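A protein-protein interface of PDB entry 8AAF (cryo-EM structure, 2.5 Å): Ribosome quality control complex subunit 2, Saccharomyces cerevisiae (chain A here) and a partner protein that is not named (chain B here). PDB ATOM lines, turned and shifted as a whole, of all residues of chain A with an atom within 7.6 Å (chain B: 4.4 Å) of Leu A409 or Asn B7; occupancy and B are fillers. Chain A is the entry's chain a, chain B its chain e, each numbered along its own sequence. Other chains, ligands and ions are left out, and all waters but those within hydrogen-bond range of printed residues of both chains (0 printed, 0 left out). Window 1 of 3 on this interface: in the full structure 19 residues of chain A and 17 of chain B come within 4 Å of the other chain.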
ATOM      1  N   LYS A 403       2.643   2.466 -16.376  1.00  0.00           N
ATOM      2  CA  LYS A 403       2.452   3.474 -17.416  1.00  0.00           C
ATOM      3  C   LYS A 403       3.429   3.302 -18.565  1.00  0.00           C
ATOM      4  O   LYS A 403       3.043   3.433 -19.731  1.00  0.00           O
ATOM      5  CB  LYS A 403       2.623   4.865 -16.830  1.00  0.00           C
ATOM      6  CG  LYS A 403       1.551   5.324 -15.896  1.00  0.00           C
ATOM      7  CD  LYS A 403       2.023   6.626 -15.349  1.00  0.00           C
ATOM      8  CE  LYS A 403       1.990   7.679 -16.420  1.00  0.00           C
ATOM      9  NZ  LYS A 403       2.358   8.951 -15.817  1.00  0.00           N
ATOM     10  N   LEU A 404       4.700   3.031 -18.254  1.00  0.00           N
ATOM     11  CA  LEU A 404       5.688   2.810 -19.302  1.00  0.00           C
ATOM     12  C   LEU A 404       5.361   1.563 -20.106  1.00  0.00           C
ATOM     13  O   LEU A 404       5.545   1.544 -21.328  1.00  0.00           O
ATOM     14  CB  LEU A 404       7.086   2.712 -18.696  1.00  0.00           C
ATOM     15  CG  LEU A 404       7.813   4.047 -18.527  1.00  0.00           C
ATOM     16  CD1 LEU A 404       9.244   3.820 -18.079  1.00  0.00           C
ATOM     17  CD2 LEU A 404       7.775   4.858 -19.813  1.00  0.00           C
ATOM     18  N   ALA A 405       4.812   0.540 -19.447  1.00  0.00           N
ATOM     19  CA  ALA A 405       4.419  -0.671 -20.156  1.00  0.00           C
ATOM     20  C   ALA A 405       3.249  -0.423 -21.106  1.00  0.00           C
ATOM     21  O   ALA A 405       3.304  -0.805 -22.286  1.00  0.00           O
ATOM     22  CB  ALA A 405       4.079  -1.765 -19.149  1.00  0.00           C
ATOM     23  N   VAL A 406       2.194   0.235 -20.617  1.00  0.00           N
ATOM     24  CA  VAL A 406       1.017   0.492 -21.447  1.00  0.00           C
ATOM     25  C   VAL A 406       1.358   1.458 -22.575  1.00  0.00           C
ATOM     26  O   VAL A 406       0.908   1.286 -23.712  1.00  0.00           O
ATOM     27  CB  VAL A 406      -0.152   1.000 -20.580  1.00  0.00           C
ATOM     28  CG1 VAL A 406      -1.380   1.303 -21.427  1.00  0.00           C
ATOM     29  CG2 VAL A 406      -0.517  -0.035 -19.538  1.00  0.00           C
ATOM     30  N   GLN A 407       2.206   2.453 -22.299  1.00  0.00           N
ATOM     31  CA  GLN A 407       2.620   3.384 -23.340  1.00  0.00           C
ATOM     32  C   GLN A 407       3.516   2.721 -24.377  1.00  0.00           C
ATOM     33  O   GLN A 407       3.451   3.075 -25.558  1.00  0.00           O
ATOM     34  CB  GLN A 407       3.329   4.583 -22.715  1.00  0.00           C
ATOM     35  CG  GLN A 407       3.462   5.767 -23.646  1.00  0.00           C
ATOM     36  CD  GLN A 407       2.191   6.579 -23.722  1.00  0.00           C
ATOM     37  OE1 GLN A 407       1.581   6.701 -24.783  1.00  0.00           O
ATOM     38  NE2 GLN A 407       1.777   7.138 -22.592  1.00  0.00           N
ATOM     39  N   GLY A 408       4.342   1.754 -23.966  1.00  0.00           N
ATOM     40  CA  GLY A 408       5.117   1.001 -24.937  1.00  0.00           C
ATOM     41  C   GLY A 408       4.248   0.145 -25.837  1.00  0.00           C
ATOM     42  O   GLY A 408       4.529   0.004 -27.030  1.00  0.00           O
ATOM     43  N   LEU A 409       3.182  -0.436 -25.283  1.00  0.00           N
ATOM     44  CA  LEU A 409       2.230  -1.148 -26.137  1.00  0.00           C
ATOM     45  C   LEU A 409       1.444  -0.198 -27.037  1.00  0.00           C
ATOM     46  O   LEU A 409       1.076  -0.568 -28.157  1.00  0.00           O
ATOM     47  CB  LEU A 409       1.282  -2.017 -25.311  1.00  0.00           C
ATOM     48  CG  LEU A 409       1.723  -3.425 -24.883  1.00  0.00           C
ATOM     49  CD1 LEU A 409       1.897  -4.233 -26.146  1.00  0.00           C
ATOM     50  CD2 LEU A 409       2.995  -3.515 -24.071  1.00  0.00           C
ATOM     51  N   ILE A 410       1.161   1.016 -26.560  1.00  0.00           N
ATOM     52  CA  ILE A 410       0.444   1.998 -27.374  1.00  0.00           C
ATOM     53  C   ILE A 410       1.307   2.475 -28.537  1.00  0.00           C
ATOM     54  O   ILE A 410       0.833   2.591 -29.675  1.00  0.00           O
ATOM     55  CB  ILE A 410      -0.039   3.163 -26.487  1.00  0.00           C
ATOM     56  CG1 ILE A 410      -1.256   2.728 -25.669  1.00  0.00           C
ATOM     57  CG2 ILE A 410      -0.345   4.415 -27.291  1.00  0.00           C
ATOM     58  CD1 ILE A 410      -1.802   3.803 -24.770  1.00  0.00           C
ATOM     59  N   ASP A 411       2.600   2.688 -28.289  1.00  0.00           N
ATOM     60  CA  ASP A 411       3.505   3.218 -29.304  1.00  0.00           C
ATOM     61  C   ASP A 411       3.819   2.225 -30.414  1.00  0.00           C
ATOM     62  O   ASP A 411       4.439   2.615 -31.408  1.00  0.00           O
ATOM     63  CB  ASP A 411       4.802   3.683 -28.652  1.00  0.00           C
ATOM     64  CG  ASP A 411       4.613   4.924 -27.812  1.00  0.00           C
ATOM     65  OD1 ASP A 411       3.541   5.555 -27.918  1.00  0.00           O
ATOM     66  OD2 ASP A 411       5.531   5.266 -27.040  1.00  0.00           O
ATOM     67  N   GLN A 412       3.410   0.967 -30.280  1.00  0.00           N
ATOM     68  CA  GLN A 412       3.487   0.001 -31.363  1.00  0.00           C
ATOM     69  C   GLN A 412       2.297   0.088 -32.305  1.00  0.00           C
ATOM     70  O   GLN A 412       2.208  -0.731 -33.228  1.00  0.00           O
ATOM     71  CB  GLN A 412       3.585  -1.417 -30.797  1.00  0.00           C
ATOM     72  CG  GLN A 412       4.784  -1.632 -29.903  1.00  0.00           C
ATOM     73  CD  GLN A 412       4.829  -3.024 -29.316  1.00  0.00           C
ATOM     74  OE1 GLN A 412       4.247  -3.960 -29.864  1.00  0.00           O
ATOM     75  NE2 GLN A 412       5.518  -3.168 -28.191  1.00  0.00           N
ATOM     76  N   GLN A 413       1.399   1.061 -32.080  1.00  0.00           N
ATOM     77  CA  GLN A 413       0.159   1.255 -32.842  1.00  0.00           C
ATOM     78  C   GLN A 413      -0.706   0.000 -32.818  1.00  0.00           C
ATOM     79  O   GLN A 413      -1.273  -0.408 -33.832  1.00  0.00           O
ATOM     80  CB  GLN A 413       0.439   1.706 -34.276  1.00  0.00           C
ATOM     81  CG  GLN A 413       0.704   3.186 -34.411  1.00  0.00           C
ATOM     82  CD  GLN A 413       0.714   3.630 -35.854  1.00  0.00           C
ATOM     83  OE1 GLN A 413       1.771   3.861 -36.435  1.00  0.00           O
ATOM     84  NE2 GLN A 413      -0.469   3.735 -36.445  1.00  0.00           N
ATOM     85  N   MET A 414      -0.783  -0.628 -31.652  1.00  0.00           N
ATOM     86  CA  MET A 414      -1.497  -1.881 -31.515  1.00  0.00           C
ATOM     87  C   MET A 414      -2.964  -1.600 -31.212  1.00  0.00           C
ATOM     88  O   MET A 414      -3.306  -0.584 -30.602  1.00  0.00           O
ATOM     89  CB  MET A 414      -0.841  -2.724 -30.417  1.00  0.00           C
ATOM     90  CG  MET A 414      -1.380  -4.129 -30.220  1.00  0.00           C
ATOM     91  SD  MET A 414      -0.508  -5.003 -28.913  1.00  0.00           S
ATOM     92  CE  MET A 414       1.064  -5.293 -29.720  1.00  0.00           C
ATOM     93  N   ASP A 415      -3.831  -2.501 -31.671  1.00  0.00           N
ATOM     94  CA  ASP A 415      -5.264  -2.365 -31.474  1.00  0.00           C
ATOM     95  C   ASP A 415      -5.614  -2.464 -29.993  1.00  0.00           C
ATOM     96  O   ASP A 415      -5.028  -3.252 -29.249  1.00  0.00           O
ATOM     97  CB  ASP A 415      -6.002  -3.443 -32.266  1.00  0.00           C
ATOM     98  CG  ASP A 415      -7.505  -3.276 -32.227  1.00  0.00           C
ATOM     99  OD1 ASP A 415      -7.981  -2.155 -31.956  1.00  0.00           O
ATOM    100  OD2 ASP A 415      -8.214  -4.273 -32.463  1.00  0.00           O
ATOM    101  N   TRP A 416      -6.582  -1.639 -29.575  1.00  0.00           N
ATOM    102  CA  TRP A 416      -6.899  -1.497 -28.155  1.00  0.00           C
ATOM    103  C   TRP A 416      -7.498  -2.769 -27.571  1.00  0.00           C
ATOM    104  O   TRP A 416      -7.189  -3.138 -26.429  1.00  0.00           O
ATOM    105  CB  TRP A 416      -7.856  -0.321 -27.949  1.00  0.00           C
ATOM    106  CG  TRP A 416      -7.240   1.021 -28.206  1.00  0.00           C
ATOM    107  CD1 TRP A 416      -5.931   1.282 -28.473  1.00  0.00           C
ATOM    108  CD2 TRP A 416      -7.904   2.291 -28.189  1.00  0.00           C
ATOM    109  NE1 TRP A 416      -5.739   2.630 -28.638  1.00  0.00           N
ATOM    110  CE2 TRP A 416      -6.935   3.271 -28.468  1.00  0.00           C
ATOM    111  CE3 TRP A 416      -9.224   2.692 -27.971  1.00  0.00           C
ATOM    112  CZ2 TRP A 416      -7.242   4.625 -28.532  1.00  0.00           C
ATOM    113  CZ3 TRP A 416      -9.526   4.038 -28.034  1.00  0.00           C
ATOM    114  CH2 TRP A 416      -8.540   4.987 -28.315  1.00  0.00           C
ATOM    115  N   THR A 418      -6.946  -5.842 -28.713  1.00  0.00           N
ATOM    116  CA  THR A 418      -5.835  -6.779 -28.617  1.00  0.00           C
ATOM    117  C   THR A 418      -4.930  -6.463 -27.434  1.00  0.00           C
ATOM    118  O   THR A 418      -4.392  -7.389 -26.818  1.00  0.00           O
ATOM    119  CB  THR A 418      -5.015  -6.767 -29.902  1.00  0.00           C
ATOM    120  OG1 THR A 418      -4.470  -5.461 -30.101  1.00  0.00           O
ATOM    121  CG2 THR A 418      -5.889  -7.108 -31.086  1.00  0.00           C
ATOM    122  N   ILE A 419      -4.780  -5.183 -27.086  1.00  0.00           N
ATOM    123  CA  ILE A 419      -4.039  -4.821 -25.882  1.00  0.00           C
ATOM    124  C   ILE A 419      -4.764  -5.311 -24.633  1.00  0.00           C
ATOM    125  O   ILE A 419      -4.130  -5.862 -23.724  1.00  0.00           O
ATOM    126  CB  ILE A 419      -3.791  -3.301 -25.844  1.00  0.00           C
ATOM    127  CG1 ILE A 419      -2.773  -2.905 -26.913  1.00  0.00           C
ATOM    128  CG2 ILE A 419      -3.298  -2.841 -24.481  1.00  0.00           C
ATOM    129  CD1 ILE A 419      -2.476  -1.418 -26.961  1.00  0.00           C
ATOM    130  N   LEU A 422      -4.242  -8.988 -24.390  1.00  0.00           N
ATOM    131  CA  LEU A 422      -2.897  -9.204 -23.874  1.00  0.00           C
ATOM    132  C   LEU A 422      -2.810  -8.967 -22.372  1.00  0.00           C
ATOM    133  O   LEU A 422      -2.045  -9.660 -21.692  1.00  0.00           O
ATOM    134  CB  LEU A 422      -1.914  -8.294 -24.610  1.00  0.00           C
ATOM    135  CG  LEU A 422      -0.432  -8.443 -24.272  1.00  0.00           C
ATOM    136  CD1 LEU A 422       0.023  -9.859 -24.525  1.00  0.00           C
ATOM    137  CD2 LEU A 422       0.396  -7.475 -25.076  1.00  0.00           C
ATOM    138  N   ILE A 423      -3.576  -8.016 -21.843  1.00  0.00           N
ATOM    139  CA  ILE A 423      -3.601  -7.808 -20.397  1.00  0.00           C
ATOM    140  C   ILE A 423      -4.274  -8.984 -19.696  1.00  0.00           C
ATOM    141  O   ILE A 423      -3.783  -9.465 -18.667  1.00  0.00           O
ATOM    142  CB  ILE A 423      -4.277  -6.468 -20.050  1.00  0.00           C
ATOM    143  CG1 ILE A 423      -3.469  -5.305 -20.617  1.00  0.00           C
ATOM    144  CG2 ILE A 423      -4.388  -6.281 -18.545  1.00  0.00           C
ATOM    145  CD1 ILE A 423      -2.062  -5.227 -20.087  1.00  0.00           C
ATOM    146  N   ILE B   6       7.893  -0.530 -27.479  1.00  0.00           N
ATOM    147  CA  ILE B   6       8.666  -1.552 -26.778  1.00  0.00           C
ATOM    148  C   ILE B   6       7.750  -2.592 -26.153  1.00  0.00           C
ATOM    149  O   ILE B   6       6.738  -2.234 -25.559  1.00  0.00           O
ATOM    150  CB  ILE B   6       9.510  -0.911 -25.661  1.00  0.00           C
ATOM    151  CG1 ILE B   6      10.571   0.021 -26.246  1.00  0.00           C
ATOM    152  CG2 ILE B   6      10.203  -1.967 -24.814  1.00  0.00           C
ATOM    153  CD1 ILE B   6      11.654  -0.702 -27.018  1.00  0.00           C
ATOM    154  N   ASN B   7       8.079  -3.873 -26.276  1.00  0.00           N
ATOM    155  CA  ASN B   7       7.280  -4.900 -25.612  1.00  0.00           C
ATOM    156  C   ASN B   7       7.727  -5.090 -24.175  1.00  0.00           C
ATOM    157  O   ASN B   7       8.325  -6.109 -23.841  1.00  0.00           O
ATOM    158  CB  ASN B   7       7.377  -6.226 -26.354  1.00  0.00           C
ATOM    159  CG  ASN B   7       6.306  -6.385 -27.411  1.00  0.00           C
ATOM    160  OD1 ASN B   7       5.166  -5.964 -27.221  1.00  0.00           O
ATOM    161  ND2 ASN B   7       6.662  -7.010 -28.526  1.00  0.00           N
ATOM    162  N   THR B   8       7.433  -4.120 -23.319  1.00  0.00           N
ATOM    163  CA  THR B   8       7.841  -4.195 -21.922  1.00  0.00           C
ATOM    164  C   THR B   8       7.191  -5.341 -21.170  1.00  0.00           C
ATOM    165  O   THR B   8       7.841  -5.994 -20.359  1.00  0.00           O
ATOM    166  CB  THR B   8       7.560  -2.882 -21.193  1.00  0.00           C
ATOM    167  OG1 THR B   8       7.213  -1.875 -22.150  1.00  0.00           O
ATOM    168  CG2 THR B   8       8.784  -2.434 -20.416  1.00  0.00           C
ATOM    169  N   PHE B   9       5.917  -5.604 -21.442  1.00  0.00           N
ATOM    170  CA  PHE B   9       5.201  -6.654 -20.727  1.00  0.00           C
ATOM    171  C   PHE B   9       5.859  -7.996 -20.956  1.00  0.00           C
ATOM    172  O   PHE B   9       5.970  -8.805 -20.037  1.00  0.00           O
ATOM    173  CB  PHE B   9       3.751  -6.724 -21.190  1.00  0.00           C
ATOM    174  CG  PHE B   9       2.813  -5.920 -20.354  1.00  0.00           C
ATOM    175  CD1 PHE B   9       2.412  -6.381 -19.118  1.00  0.00           C
ATOM    176  CD2 PHE B   9       2.328  -4.709 -20.802  1.00  0.00           C
ATOM    177  CE1 PHE B   9       1.546  -5.646 -18.343  1.00  0.00           C
ATOM    178  CE2 PHE B   9       1.459  -3.968 -20.031  1.00  0.00           C
ATOM    179  CZ  PHE B   9       1.072  -4.435 -18.795  1.00  0.00           C
ATOM    180  N   GLN B  10       6.309  -8.235 -22.177  1.00  0.00           N
ATOM    181  CA  GLN B  10       6.929  -9.509 -22.511  1.00  0.00           C
ATOM    182  C   GLN B  10       8.195  -9.776 -21.721  1.00  0.00           C
ATOM    183  O   GLN B  10       8.471 -10.918 -21.366  1.00  0.00           O
ATOM    184  CB  GLN B  10       7.212  -9.582 -24.009  1.00  0.00           C
ATOM    185  CG  GLN B  10       5.985  -9.334 -24.873  1.00  0.00           C
ATOM    186  CD  GLN B  10       4.884 -10.354 -24.654  1.00  0.00           C
ATOM    187  OE1 GLN B  10       5.146 -11.543 -24.465  1.00  0.00           O
ATOM    188  NE2 GLN B  10       3.640  -9.894 -24.694  1.00  0.00           N
ATOM    189  N   GLN B  11       8.970  -8.738 -21.443  1.00  0.00           N
ATOM    190  CA  GLN B  11      10.242  -8.934 -20.762  1.00  0.00           C
ATOM    191  C   GLN B  11      10.053  -9.580 -19.408  1.00  0.00           C
ATOM    192  O   GLN B  11      10.831 -10.444 -19.016  1.00  0.00           O
ATOM    193  CB  GLN B  11      10.924  -7.589 -20.564  1.00  0.00           C
ATOM    194  CG  GLN B  11      11.070  -6.783 -21.840  1.00  0.00           C
ATOM    195  CD  GLN B  11      11.369  -5.325 -21.567  1.00  0.00           C
ATOM    196  OE1 GLN B  11      11.424  -4.898 -20.414  1.00  0.00           O
ATOM    197  NE2 GLN B  11      11.555  -4.550 -22.628  1.00  0.00           N
ATOM    198  N   LEU B  33       4.098 -11.334 -31.456  1.00  0.00           N
ATOM    199  CA  LEU B  33       4.329 -10.476 -32.603  1.00  0.00           C
ATOM    200  C   LEU B  33       5.755  -9.990 -32.563  1.00  0.00           C
ATOM    201  O   LEU B  33       6.310  -9.795 -31.489  1.00  0.00           O
ATOM    202  CB  LEU B  33       3.366  -9.304 -32.554  1.00  0.00           C
ATOM    203  CG  LEU B  33       1.905  -9.645 -32.824  1.00  0.00           C
ATOM    204  CD1 LEU B  33       1.005  -8.490 -32.417  1.00  0.00           C
ATOM    205  CD2 LEU B  33       1.722  -9.985 -34.293  1.00  0.00           C
ATOM    206  N   ASP B  35       9.092  -8.038 -32.202  1.00  0.00           N
ATOM    207  CA  ASP B  35       9.403  -6.835 -31.436  1.00  0.00           C
ATOM    208  C   ASP B  35       9.794  -5.711 -32.351  1.00  0.00           C
ATOM    209  O   ASP B  35      10.483  -5.932 -33.337  1.00  0.00           O
ATOM    210  CB  ASP B  35      10.564  -7.120 -30.494  1.00  0.00           C
ATOM    211  CG  ASP B  35      10.682  -6.102 -29.385  1.00  0.00           C
ATOM    212  OD1 ASP B  35       9.677  -5.869 -28.688  1.00  0.00           O
ATOM    213  OD2 ASP B  35      11.782  -5.544 -29.200  1.00  0.00           O
ATOM    214  N   PRO B  36       9.394  -4.490 -32.021  1.00  0.00           N
ATOM    215  CA  PRO B  36       9.687  -3.416 -32.957  1.00  0.00           C
ATOM    216  C   PRO B  36      11.171  -3.201 -33.209  1.00  0.00           C
ATOM    217  O   PRO B  36      11.565  -2.920 -34.336  1.00  0.00           O
ATOM    218  CB  PRO B  36       9.091  -2.217 -32.260  1.00  0.00           C
ATOM    219  CG  PRO B  36       7.882  -2.779 -31.607  1.00  0.00           C
ATOM    220  CD  PRO B  36       8.327  -4.110 -31.081  1.00  0.00           C
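The backbone carbonyl oxygen (O) of Gly A408 is in hydrogen-bond range of the backbone NH (N) of Ile B6, 3.4 Å away. The side-chain amide nitrogen (NE2) of Gln A412 sits at hydrogen-bond distance from the side-chain amide oxygen (OD1) of Asn B7. The backbone carbonyl oxygen of Ile B6 is in hydrogen-bond range of the side-chain amide nitrogen of Gln A412, 3.0 Å away.
ND2 of Asn B7 is in hydrogen-bond range of OD1 of Asp B35 (3.2 Å). OG1 of Thr B8 lies within hydrogen-bond range of O of Ile B6, at 3.5 Å.
OG1 of Thr B8 touches O of Leu A404, 3.9 Å away. Ala A405 touches Thr B8. Ala A405 touches Phe B9. Ile B6 touches Leu A409 (O to N, 3.99 Å). CD1 of Leu A409 touches OD1 of Asn B7, 3.9 Å away. Phe B9 touches Leu A409 (CD2 to CD2, 3.5 Å). Pro B36 touches Gln A412 (CG to CG, 3.7 Å). Gln B10 touches Leu A422. CD1 of Ile A423 touches CZ of Phe B9, 3.5 Å away.
Of the printed residues of chain A, Asn B7 touches Leu A409 and Gln A412. Of the printed residues of chain B, Gln A412 touches Ile B6 (3.0 Å), Asn B7 (3.0 Å) and Pro B36 (3.7 Å). Of the printed residues of chain B, Ile A423 touches Phe B9 (3.5 Å). Of the printed residues of chain B, Leu A404 touches Thr B8. Of the printed residues of chain B, Ala A405 touches Thr B8 and Phe B9. Printed residues of chain B within 4 Å of Gly A408: Ile B6 (3.4 Å). The nearest printed residue of chain B that does not touch Leu A409 is Thr B8 (4.5 Å). The nearest residue of chain A that does not touch Asn B7 is Met A414 (4.8 Å). The nearest printed residue of chain A that does not touch Pro B36 is Gly A408 (6.3 Å).
Of the 18 printed residues of chain A, 7 touch a printed residue of chain B. Hydrophobic or aromatic side chains of chain A that line the printed part of chain B: Ala A405, Leu A409, Leu A422 and Ile A423. Among the printed residues, 12 pairs touch across the chains.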
